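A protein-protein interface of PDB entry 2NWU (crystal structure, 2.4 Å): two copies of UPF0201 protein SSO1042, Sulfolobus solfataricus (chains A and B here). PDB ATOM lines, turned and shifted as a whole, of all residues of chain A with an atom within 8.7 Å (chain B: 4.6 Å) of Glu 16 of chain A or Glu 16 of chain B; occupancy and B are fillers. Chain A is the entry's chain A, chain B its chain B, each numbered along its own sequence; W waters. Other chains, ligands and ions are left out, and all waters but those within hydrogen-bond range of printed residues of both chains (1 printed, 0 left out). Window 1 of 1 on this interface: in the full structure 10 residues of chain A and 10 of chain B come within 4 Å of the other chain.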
ATOM      1  N   ALA A  10       3.220  -7.574  19.941  1.00  0.00           N
ATOM      2  CA  ALA A  10       4.480  -8.214  20.267  1.00  0.00           C
ATOM      3  C   ALA A  10       4.239  -9.602  20.841  1.00  0.00           C
ATOM      4  O   ALA A  10       3.239  -9.844  21.523  1.00  0.00           O
ATOM      5  CB  ALA A  10       5.242  -7.361  21.272  1.00  0.00           C
ATOM      6  N   GLU A  11       5.161 -10.515  20.564  1.00  0.00           N
ATOM      7  CA  GLU A  11       5.045 -11.871  21.075  1.00  0.00           C
ATOM      8  C   GLU A  11       5.705 -11.971  22.438  1.00  0.00           C
ATOM      9  O   GLU A  11       6.676 -11.271  22.731  1.00  0.00           O
ATOM     10  CB  GLU A  11       5.733 -12.870  20.141  1.00  0.00           C
ATOM     11  CG  GLU A  11       5.190 -12.963  18.720  1.00  0.00           C
ATOM     12  CD  GLU A  11       6.062 -13.867  17.839  1.00  0.00           C
ATOM     13  OE1 GLU A  11       6.229 -15.056  18.180  1.00  0.00           O
ATOM     14  OE2 GLU A  11       6.590 -13.393  16.810  1.00  0.00           O
ATOM     15  N   VAL A  12       5.166 -12.843  23.275  1.00  0.00           N
ATOM     16  CA  VAL A  12       5.746 -13.087  24.585  1.00  0.00           C
ATOM     17  C   VAL A  12       5.925 -14.597  24.682  1.00  0.00           C
ATOM     18  O   VAL A  12       4.957 -15.329  24.895  1.00  0.00           O
ATOM     19  CB  VAL A  12       4.830 -12.623  25.723  1.00  0.00           C
ATOM     20  CG1 VAL A  12       5.528 -12.860  27.062  1.00  0.00           C
ATOM     21  CG2 VAL A  12       4.479 -11.137  25.543  1.00  0.00           C
ATOM     22  N   ARG A  13       7.152 -15.065  24.480  1.00  0.00           N
ATOM     23  CA  ARG A  13       7.433 -16.490  24.560  1.00  0.00           C
ATOM     24  C   ARG A  13       7.482 -16.938  26.011  1.00  0.00           C
ATOM     25  O   ARG A  13       7.616 -16.122  26.919  1.00  0.00           O
ATOM     26  CB  ARG A  13       8.772 -16.823  23.908  1.00  0.00           C
ATOM     27  CG  ARG A  13       8.895 -16.414  22.452  1.00  0.00           C
ATOM     28  CD  ARG A  13       7.720 -16.877  21.641  1.00  0.00           C
ATOM     29  NE  ARG A  13       7.890 -16.500  20.245  1.00  0.00           N
ATOM     30  CZ  ARG A  13       8.629 -17.181  19.379  1.00  0.00           C
ATOM     31  NH1 ARG A  13       9.256 -18.279  19.772  1.00  0.00           N
ATOM     32  NH2 ARG A  13       8.747 -16.758  18.128  1.00  0.00           N
ATOM     33  N   PRO A  14       7.370 -18.251  26.244  1.00  0.00           N
ATOM     34  CA  PRO A  14       7.402 -18.836  27.586  1.00  0.00           C
ATOM     35  C   PRO A  14       8.655 -18.430  28.360  1.00  0.00           C
ATOM     36  O   PRO A  14       8.630 -18.367  29.587  1.00  0.00           O
ATOM     37  CB  PRO A  14       7.357 -20.333  27.308  1.00  0.00           C
ATOM     38  CG  PRO A  14       6.564 -20.414  26.046  1.00  0.00           C
ATOM     39  CD  PRO A  14       7.114 -19.284  25.225  1.00  0.00           C
ATOM     40  N   SER A  15       9.746 -18.159  27.638  1.00  0.00           N
ATOM     41  CA  SER A  15      10.999 -17.745  28.274  1.00  0.00           C
ATOM     42  C   SER A  15      11.078 -16.234  28.500  1.00  0.00           C
ATOM     43  O   SER A  15      11.985 -15.765  29.178  1.00  0.00           O
ATOM     44  CB  SER A  15      12.215 -18.208  27.448  1.00  0.00           C
ATOM     45  OG  SER A  15      12.485 -17.373  26.335  1.00  0.00           O
ATOM     46  N   GLU A  16      10.121 -15.480  27.960  1.00  0.00           N
ATOM     47  CA  GLU A  16      10.117 -14.017  28.115  1.00  0.00           C
ATOM     48  C   GLU A  16       9.247 -13.493  29.262  1.00  0.00           C
ATOM     49  O   GLU A  16       8.338 -14.178  29.736  1.00  0.00           O
ATOM     50  CB  GLU A  16       9.649 -13.337  26.819  1.00  0.00           C
ATOM     51  CG  GLU A  16      10.482 -13.669  25.602  1.00  0.00           C
ATOM     52  CD  GLU A  16      10.032 -12.908  24.373  1.00  0.00           C
ATOM     53  OE1 GLU A  16      10.582 -11.815  24.104  1.00  0.00           O
ATOM     54  OE2 GLU A  16       9.119 -13.407  23.684  1.00  0.00           O
ATOM     55  N   ASP A  17       9.534 -12.273  29.705  1.00  0.00           N
ATOM     56  CA  ASP A  17       8.746 -11.660  30.766  1.00  0.00           C
ATOM     57  C   ASP A  17       7.894 -10.557  30.132  1.00  0.00           C
ATOM     58  O   ASP A  17       8.418  -9.579  29.608  1.00  0.00           O
ATOM     59  CB  ASP A  17       9.661 -11.084  31.860  1.00  0.00           C
ATOM     60  CG  ASP A  17       8.879 -10.504  33.030  1.00  0.00           C
ATOM     61  OD1 ASP A  17       7.998 -11.202  33.584  1.00  0.00           O
ATOM     62  OD2 ASP A  17       9.151  -9.341  33.402  1.00  0.00           O
ATOM     63  N   VAL A  18       6.577 -10.735  30.169  1.00  0.00           N
ATOM     64  CA  VAL A  18       5.647  -9.773  29.587  1.00  0.00           C
ATOM     65  C   VAL A  18       5.953  -8.357  30.071  1.00  0.00           C
ATOM     66  O   VAL A  18       5.771  -7.383  29.343  1.00  0.00           O
ATOM     67  CB  VAL A  18       4.187 -10.156  29.933  1.00  0.00           C
ATOM     68  CG1 VAL A  18       3.985 -10.131  31.443  1.00  0.00           C
ATOM     69  CG2 VAL A  18       3.215  -9.221  29.221  1.00  0.00           C
ATOM     70  N   ASN A  19       6.434  -8.243  31.301  1.00  0.00           N
ATOM     71  CA  ASN A  19       6.775  -6.939  31.846  1.00  0.00           C
ATOM     72  C   ASN A  19       7.973  -6.318  31.128  1.00  0.00           C
ATOM     73  O   ASN A  19       8.023  -5.105  30.950  1.00  0.00           O
ATOM     74  CB  ASN A  19       7.031  -7.052  33.347  1.00  0.00           C
ATOM     75  CG  ASN A  19       5.754  -7.342  34.119  1.00  0.00           C
ATOM     76  OD1 ASN A  19       4.789  -6.595  34.025  1.00  0.00           O
ATOM     77  ND2 ASN A  19       5.736  -8.431  34.869  1.00  0.00           N
ATOM     78  N   LYS A  20       8.931  -7.141  30.702  1.00  0.00           N
ATOM     79  CA  LYS A  20      10.084  -6.610  29.987  1.00  0.00           C
ATOM     80  C   LYS A  20       9.663  -6.183  28.582  1.00  0.00           C
ATOM     81  O   LYS A  20      10.169  -5.196  28.043  1.00  0.00           O
ATOM     82  CB  LYS A  20      11.210  -7.638  29.927  1.00  0.00           C
ATOM     83  CG  LYS A  20      11.766  -7.971  31.308  1.00  0.00           C
ATOM     84  CD  LYS A  20      13.073  -8.747  31.233  1.00  0.00           C
ATOM     85  CE  LYS A  20      13.417  -9.372  32.577  1.00  0.00           C
ATOM     86  NZ  LYS A  20      13.488  -8.360  33.673  1.00  0.00           N
ATOM     87  N   VAL A  21       8.722  -6.917  27.995  1.00  0.00           N
ATOM     88  CA  VAL A  21       8.234  -6.570  26.669  1.00  0.00           C
ATOM     89  C   VAL A  21       7.373  -5.300  26.742  1.00  0.00           C
ATOM     90  O   VAL A  21       7.435  -4.445  25.859  1.00  0.00           O
ATOM     91  CB  VAL A  21       7.410  -7.707  26.070  1.00  0.00           C
ATOM     92  CG1 VAL A  21       6.830  -7.275  24.730  1.00  0.00           C
ATOM     93  CG2 VAL A  21       8.291  -8.942  25.903  1.00  0.00           C
ATOM     94  N   LEU A  22       6.564  -5.175  27.794  1.00  0.00           N
ATOM     95  CA  LEU A  22       5.728  -3.982  27.964  1.00  0.00           C
ATOM     96  C   LEU A  22       6.615  -2.771  28.231  1.00  0.00           C
ATOM     97  O   LEU A  22       6.344  -1.666  27.758  1.00  0.00           O
ATOM     98  CB  LEU A  22       4.750  -4.167  29.127  1.00  0.00           C
ATOM     99  CG  LEU A  22       3.581  -5.116  28.830  1.00  0.00           C
ATOM    100  CD1 LEU A  22       2.890  -5.546  30.131  1.00  0.00           C
ATOM    101  CD2 LEU A  22       2.607  -4.413  27.887  1.00  0.00           C
ATOM    102  N   ALA A  24       9.653  -2.446  27.147  1.00  0.00           N
ATOM    103  CA  ALA A  24      10.287  -2.185  25.852  1.00  0.00           C
ATOM    104  C   ALA A  24       9.420  -1.256  24.997  1.00  0.00           C
ATOM    105  O   ALA A  24       9.905  -0.296  24.387  1.00  0.00           O
ATOM    106  CB  ALA A  24      10.495  -3.501  25.097  1.00  0.00           C
ATOM    107  N   ILE A  41       1.940 -22.028  22.280  1.00  0.00           N
ATOM    108  CA  ILE A  41       2.502 -21.780  23.598  1.00  0.00           C
ATOM    109  C   ILE A  41       3.030 -20.352  23.706  1.00  0.00           C
ATOM    110  O   ILE A  41       3.602 -19.970  24.731  1.00  0.00           O
ATOM    111  CB  ILE A  41       3.640 -22.774  23.924  1.00  0.00           C
ATOM    112  CG1 ILE A  41       4.758 -22.668  22.882  1.00  0.00           C
ATOM    113  CG2 ILE A  41       3.089 -24.189  23.945  1.00  0.00           C
ATOM    114  CD1 ILE A  41       6.005 -23.450  23.247  1.00  0.00           C
ATOM    115  N   ILE A  42       2.818 -19.562  22.653  1.00  0.00           N
ATOM    116  CA  ILE A  42       3.276 -18.176  22.625  1.00  0.00           C
ATOM    117  C   ILE A  42       2.134 -17.163  22.745  1.00  0.00           C
ATOM    118  O   ILE A  42       1.127 -17.248  22.040  1.00  0.00           O
ATOM    119  CB  ILE A  42       4.076 -17.874  21.327  1.00  0.00           C
ATOM    120  CG1 ILE A  42       3.159 -17.919  20.106  1.00  0.00           C
ATOM    121  CG2 ILE A  42       5.180 -18.909  21.144  1.00  0.00           C
ATOM    122  CD1 ILE A  42       3.899 -17.738  18.790  1.00  0.00           C
ATOM    123  N   ASP A  43       2.297 -16.203  23.648  1.00  0.00           N
ATOM    124  CA  ASP A  43       1.290 -15.165  23.844  1.00  0.00           C
ATOM    125  C   ASP A  43       1.493 -14.007  22.861  1.00  0.00           C
ATOM    126  O   ASP A  43       2.613 -13.712  22.442  1.00  0.00           O
ATOM    127  CB  ASP A  43       1.359 -14.632  25.279  1.00  0.00           C
ATOM    128  CG  ASP A  43       0.848 -15.629  26.290  1.00  0.00           C
ATOM    129  OD1 ASP A  43       1.155 -16.830  26.131  1.00  0.00           O
ATOM    130  OD2 ASP A  43       0.150 -15.217  27.243  1.00  0.00           O
ATOM    131  N   LYS A  90      13.016  -5.872  18.839  1.00  0.00           N
ATOM    132  CA  LYS A  90      12.579  -6.230  20.176  1.00  0.00           C
ATOM    133  C   LYS A  90      13.656  -6.044  21.259  1.00  0.00           C
ATOM    134  O   LYS A  90      13.486  -5.260  22.194  1.00  0.00           O
ATOM    135  CB  LYS A  90      12.137  -7.689  20.157  1.00  0.00           C
ATOM    136  CG  LYS A  90      11.553  -8.211  21.440  1.00  0.00           C
ATOM    137  CD  LYS A  90      10.041  -8.201  21.355  1.00  0.00           C
ATOM    138  CE  LYS A  90       9.439  -9.295  22.217  1.00  0.00           C
ATOM    139  NZ  LYS A  90       9.756 -10.633  21.650  1.00  0.00           N
ATOM    140  N   GLN A  91      14.756  -6.777  21.138  1.00  0.00           N
ATOM    141  CA  GLN A  91      15.814  -6.699  22.139  1.00  0.00           C
ATOM    142  C   GLN A  91      16.402  -5.295  22.283  1.00  0.00           C
ATOM    143  O   GLN A  91      16.687  -4.851  23.394  1.00  0.00           O
ATOM    144  CB  GLN A  91      16.924  -7.708  21.820  1.00  0.00           C
ATOM    145  CG  GLN A  91      16.468  -9.180  21.750  1.00  0.00           C
ATOM    146  CD  GLN A  91      15.603  -9.615  22.936  1.00  0.00           C
ATOM    147  OE1 GLN A  91      15.930  -9.350  24.105  1.00  0.00           O
ATOM    148  NE2 GLN A  91      14.496 -10.294  22.638  1.00  0.00           N
ATOM    149  N   ALA A  94      14.057  -3.358  24.179  1.00  0.00           N
ATOM    150  CA  ALA A  94      14.026  -3.769  25.583  1.00  0.00           C
ATOM    151  C   ALA A  94      15.078  -2.969  26.364  1.00  0.00           C
ATOM    152  O   ALA A  94      14.886  -2.671  27.543  1.00  0.00           O
ATOM    153  CB  ALA A  94      14.284  -5.263  25.709  1.00  0.00           C
ATOM    154  N   ALA A 111      10.417  -7.642  15.672  1.00  0.00           N
ATOM    155  CA  ALA A 111       9.358  -8.427  16.297  1.00  0.00           C
ATOM    156  C   ALA A 111       8.302  -7.557  16.989  1.00  0.00           C
ATOM    157  O   ALA A 111       7.258  -8.063  17.379  1.00  0.00           O
ATOM    158  CB  ALA A 111       9.957  -9.439  17.283  1.00  0.00           C
ATOM    159  N   ILE A 112       8.571  -6.264  17.177  1.00  0.00           N
ATOM    160  CA  ILE A 112       7.555  -5.374  17.764  1.00  0.00           C
ATOM    161  C   ILE A 112       6.910  -4.630  16.581  1.00  0.00           C
ATOM    162  O   ILE A 112       7.541  -3.783  15.940  1.00  0.00           O
ATOM    163  CB  ILE A 112       8.153  -4.352  18.756  1.00  0.00           C
ATOM    164  CG1 ILE A 112       8.676  -5.080  20.004  1.00  0.00           C
ATOM    165  CG2 ILE A 112       7.089  -3.348  19.164  1.00  0.00           C
ATOM    166  CD1 ILE A 112       9.309  -4.169  21.061  1.00  0.00           C
ATOM    167  N   GLU B  11      21.225 -18.813  26.455  1.00  0.00           N
ATOM    168  CA  GLU B  11      21.273 -17.362  26.476  1.00  0.00           C
ATOM    169  C   GLU B  11      20.036 -16.779  27.130  1.00  0.00           C
ATOM    170  O   GLU B  11      19.000 -17.438  27.242  1.00  0.00           O
ATOM    171  CB  GLU B  11      21.386 -16.789  25.061  1.00  0.00           C
ATOM    172  CG  GLU B  11      22.516 -17.348  24.211  1.00  0.00           C
ATOM    173  CD  GLU B  11      22.207 -18.728  23.680  1.00  0.00           C
ATOM    174  OE1 GLU B  11      21.082 -18.911  23.171  1.00  0.00           O
ATOM    175  OE2 GLU B  11      23.081 -19.623  23.764  1.00  0.00           O
ATOM    176  N   VAL B  12      20.173 -15.537  27.579  1.00  0.00           N
ATOM    177  CA  VAL B  12      19.081 -14.793  28.186  1.00  0.00           C
ATOM    178  C   VAL B  12      19.146 -13.406  27.560  1.00  0.00           C
ATOM    179  O   VAL B  12      20.065 -12.630  27.833  1.00  0.00           O
ATOM    180  CB  VAL B  12      19.232 -14.668  29.719  1.00  0.00           C
ATOM    181  CG1 VAL B  12      18.088 -13.837  30.285  1.00  0.00           C
ATOM    182  CG2 VAL B  12      19.246 -16.055  30.364  1.00  0.00           C
ATOM    183  N   ARG B  13      18.190 -13.111  26.688  1.00  0.00           N
ATOM    184  CA  ARG B  13      18.135 -11.815  26.026  1.00  0.00           C
ATOM    185  C   ARG B  13      17.433 -10.839  26.970  1.00  0.00           C
ATOM    186  O   ARG B  13      16.847 -11.254  27.975  1.00  0.00           O
ATOM    187  CB  ARG B  13      17.338 -11.918  24.731  1.00  0.00           C
ATOM    188  CG  ARG B  13      18.152 -11.830  23.474  1.00  0.00           C
ATOM    189  CD  ARG B  13      18.753 -13.158  23.091  1.00  0.00           C
ATOM    190  NE  ARG B  13      19.260 -13.120  21.723  1.00  0.00           N
ATOM    191  CZ  ARG B  13      19.850 -14.144  21.112  1.00  0.00           C
ATOM    192  NH1 ARG B  13      20.018 -15.306  21.746  1.00  0.00           N
ATOM    193  NH2 ARG B  13      20.274 -14.001  19.859  1.00  0.00           N
ATOM    194  N   PRO B  14      17.481  -9.530  26.654  1.00  0.00           N
ATOM    195  CA  PRO B  14      16.851  -8.487  27.467  1.00  0.00           C
ATOM    196  C   PRO B  14      15.343  -8.660  27.698  1.00  0.00           C
ATOM    197  O   PRO B  14      14.810  -8.190  28.703  1.00  0.00           O
ATOM    198  CB  PRO B  14      17.186  -7.211  26.693  1.00  0.00           C
ATOM    199  CG  PRO B  14      18.544  -7.521  26.135  1.00  0.00           C
ATOM    200  CD  PRO B  14      18.359  -8.930  25.626  1.00  0.00           C
ATOM    201  N   SER B  15      14.649  -9.317  26.772  1.00  0.00           N
ATOM    202  CA  SER B  15      13.207  -9.526  26.938  1.00  0.00           C
ATOM    203  C   SER B  15      12.932 -10.818  27.712  1.00  0.00           C
ATOM    204  O   SER B  15      11.793 -11.116  28.062  1.00  0.00           O
ATOM    205  CB  SER B  15      12.499  -9.594  25.580  1.00  0.00           C
ATOM    206  OG  SER B  15      12.866 -10.757  24.868  1.00  0.00           O
ATOM    207  N   GLU B  16      13.981 -11.585  27.987  1.00  0.00           N
ATOM    208  CA  GLU B  16      13.792 -12.825  28.714  1.00  0.00           C
ATOM    209  C   GLU B  16      14.019 -12.695  30.209  1.00  0.00           C
ATOM    210  O   GLU B  16      14.717 -11.796  30.683  1.00  0.00           O
ATOM    211  CB  GLU B  16      14.699 -13.916  28.157  1.00  0.00           C
ATOM    212  CG  GLU B  16      14.527 -14.159  26.674  1.00  0.00           C
ATOM    213  CD  GLU B  16      15.411 -15.291  26.167  1.00  0.00           C
ATOM    214  OE1 GLU B  16      14.946 -16.456  26.149  1.00  0.00           O
ATOM    215  OE2 GLU B  16      16.570 -15.005  25.803  1.00  0.00           O
ATOM    216  N   ASP B  17      13.405 -13.611  30.945  1.00  0.00           N
ATOM    217  CA  ASP B  17      13.534 -13.637  32.385  1.00  0.00           C
ATOM    218  C   ASP B  17      14.516 -14.753  32.694  1.00  0.00           C
ATOM    219  O   ASP B  17      14.247 -15.925  32.429  1.00  0.00           O
ATOM    220  CB  ASP B  17      12.175 -13.922  33.025  1.00  0.00           C
ATOM    221  CG  ASP B  17      12.220 -13.880  34.527  1.00  0.00           C
ATOM    222  OD1 ASP B  17      11.155 -14.083  35.141  1.00  0.00           O
ATOM    223  OD2 ASP B  17      13.304 -13.644  35.106  1.00  0.00           O
ATOM    224  N   VAL B  18      15.669 -14.381  33.233  1.00  0.00           N
ATOM    225  CA  VAL B  18      16.681 -15.359  33.570  1.00  0.00           C
ATOM    226  C   VAL B  18      16.089 -16.531  34.358  1.00  0.00           C
ATOM    227  O   VAL B  18      16.501 -17.678  34.167  1.00  0.00           O
ATOM    228  CB  VAL B  18      17.838 -14.707  34.382  1.00  0.00           C
ATOM    229  CG1 VAL B  18      17.277 -13.957  35.574  1.00  0.00           C
ATOM    230  CG2 VAL B  18      18.832 -15.774  34.847  1.00  0.00           C
ATOM    231  N   LYS B  20      13.061 -17.842  34.153  1.00  0.00           N
ATOM    232  CA  LYS B  20      12.242 -18.715  33.334  1.00  0.00           C
ATOM    233  C   LYS B  20      13.163 -19.635  32.537  1.00  0.00           C
ATOM    234  O   LYS B  20      12.832 -20.787  32.298  1.00  0.00           O
ATOM    235  CB  LYS B  20      11.329 -17.900  32.409  1.00  0.00           C
ATOM    236  CG  LYS B  20      10.154 -17.296  33.169  1.00  0.00           C
ATOM    237  CD  LYS B  20       9.230 -16.460  32.311  1.00  0.00           C
ATOM    238  CE  LYS B  20       8.049 -16.002  33.162  1.00  0.00           C
ATOM    239  NZ  LYS B  20       7.120 -15.090  32.453  1.00  0.00           N
ATOM    240  N   VAL B  21      14.329 -19.133  32.135  1.00  0.00           N
ATOM    241  CA  VAL B  21      15.273 -19.961  31.395  1.00  0.00           C
ATOM    242  C   VAL B  21      15.810 -21.043  32.353  1.00  0.00           C
ATOM    243  O   VAL B  21      15.823 -22.232  32.017  1.00  0.00           O
ATOM    244  CB  VAL B  21      16.451 -19.129  30.838  1.00  0.00           C
ATOM    245  CG1 VAL B  21      17.416 -20.034  30.073  1.00  0.00           C
ATOM    246  CG2 VAL B  21      15.928 -18.038  29.937  1.00  0.00           C
ATOM    247  N   LYS B  90      14.259 -24.482  23.465  1.00  0.00           N
ATOM    248  CA  LYS B  90      14.113 -23.666  24.665  1.00  0.00           C
ATOM    249  C   LYS B  90      12.676 -23.383  25.112  1.00  0.00           C
ATOM    250  O   LYS B  90      12.359 -23.530  26.305  1.00  0.00           O
ATOM    251  CB  LYS B  90      14.837 -22.323  24.506  1.00  0.00           C
ATOM    252  CG  LYS B  90      14.480 -21.324  25.620  1.00  0.00           C
ATOM    253  CD  LYS B  90      15.016 -19.924  25.370  1.00  0.00           C
ATOM    254  CE  LYS B  90      16.455 -19.790  25.791  1.00  0.00           C
ATOM    255  NZ  LYS B  90      16.884 -18.362  25.751  1.00  0.00           N
HETATM  256  O   HOH W   1       5.379 -13.580  31.075  1.00  0.00           O
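OG of Ser 15 of chain A sits at hydrogen-bond distance from OE1 of Glu 16 of chain B (2.6 Å). N of Asp 17 of chain B is in hydrogen-bond range of O of Ser 15 of chain A (3.1 Å). The side-chain carboxylate (OE1) of Glu 16 of chain A is in hydrogen-bond range of the side-chain hydroxyl (OG) of Ser 15 of chain B, 2.6 Å away. NZ of Lys 20 of chain B sits at hydrogen-bond distance from O of Glu 16 of chain A (3.1 Å). The backbone carbonyl oxygen (O) of Ser 15 of chain B is in hydrogen-bond range of the backbone NH (N) of Asp 17 of chain A, 3.0 Å away. The side-chain amide nitrogen (NE2) of Gln 91 of chain A lies within hydrogen-bond range of the side-chain hydroxyl (OG) of Ser 15 of chain B (2.8 Å). The side-chain amide oxygen (OE1) of Gln 91 of chain A sits close to the backbone nitrogen (N) of Pro 14 of chain B (3.0 Å).
OE2 of Glu 16 of chain A lies within hydrogen-bond range of N of Arg 13 of chain A, 2.7 Å away. The side-chain carboxylate (OE1) of Glu 16 of chain A is in salt-bridge range of the side-chain amino group (NZ) of Lys 90 of chain A. The side-chain carboxylate (OD2) of Asp 17 of chain A sits at hydrogen-bond distance from the backbone NH (N) of Lys 20 of chain A, 3.5 Å away. O of Glu 11 of chain B lies within hydrogen-bond range of NZ of Lys 90 of chain B. OE2 of Glu 16 of chain B sits at hydrogen-bond distance from N of Arg 13 of chain B, at 2.6 Å. OE1 of Glu 16 of chain B lies within salt-bridge range of NZ of Lys 90 of chain B, 2.7 Å away.
O of Pro 14 of chain A touches CD of Lys 20 of chain B (3.4 Å). Lys 20 of chain B touches Ser 15 of chain A (CB to O, 3.9 Å). Ser 15 of chain A touches Lys 90 of chain B. CA of Glu 16 of chain A touches CA of Glu 16 of chain B (3.9 Å). Asp 17 of chain A touches Asp 17 of chain B (CB to CB, 3.97 Å). Lys 20 of chain A touches Pro 14 of chain B. CB of Lys 20 of chain A touches O of Ser 15 of chain B, at 3.99 Å. Lys 20 of chain A touches Glu 16 of chain B. OE1 of Gln 91 of chain A touches CB of Arg 13 of chain B, at 3.0 Å. Ala 94 of chain A touches Pro 14 of chain B (CB to CB, 3.6 Å).
Of the printed residues of chain B, Pro 14 of chain A touches Lys 20. Of the printed residues of chain B, Ser 15 of chain A touches Glu 16 (2.6 Å), Asp 17 (3.1 Å), Lys 20 (3.9 Å) and Lys 90 (3.7 Å). Of the printed residues of chain B, Ala 94 of chain A touches Pro 14. Printed residues of chain A within 4 Å of Glu 16 of chain B: Ser 15 (2.6 Å), Glu 16 (3.9 Å) and Lys 20 (3.3 Å). Printed residues of chain A within 4 Å of Lys 20 of chain B: Pro 14, Ser 15 and Glu 16. Printed residues of chain A within 4 Å of Lys 90 of chain B: Ser 15. The nearest residue of chain A that does not touch Glu 16 of chain B is Asp 17 of chain A (4.4 Å). The nearest printed residue of chain B that does not touch Asp 17 of chain A is Lys 20 of chain B (4.1 Å).
Of the 22 printed residues of chain A, 7 touch a printed residue of chain B. Hydrophobic or aromatic side chains of chain A that line the printed part of chain B: Ala 94. Of the 11 printed residues of chain B, 7 touch a printed residue of chain A. Hydrophobic or aromatic side chains of chain B within 4 Å of the printed part of chain A: Pro 14. Among the printed residues, 17 pairs touch across the chains.
Pro 14 of chain A touches Lys 20 of chain B, and with the chains exchanged Lys 20 of chain A touches Pro 14 of chain B. Ser 15 of chain A touches Lys 90 of chain B, but with the chains exchanged Lys 90 of chain A does not touch Ser 15 of chain B (4.5 Å). Glu 16 of chain A touches Lys 20 of chain B, and with the chains exchanged Lys 20 of chain A touches Glu 16 of chain B. Asp 17 of chain B touches its own counterpart, Asp 17 of chain A. Positions printed for both chains: 11, 12, 13, 14, 15, 16, 17, 18, 20, 21 and 90. Of the 17 pairs that touch across the chains among the printed residues, 12 have their exchanged pair printed and touching as well.
Water W1 lies within hydrogen-bond range of the side-chain amino group of Lys 20 of chain B, the backbone NH of Val 18 of chain A and the backbone carbonyl oxygen of Glu 16 of chain A.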
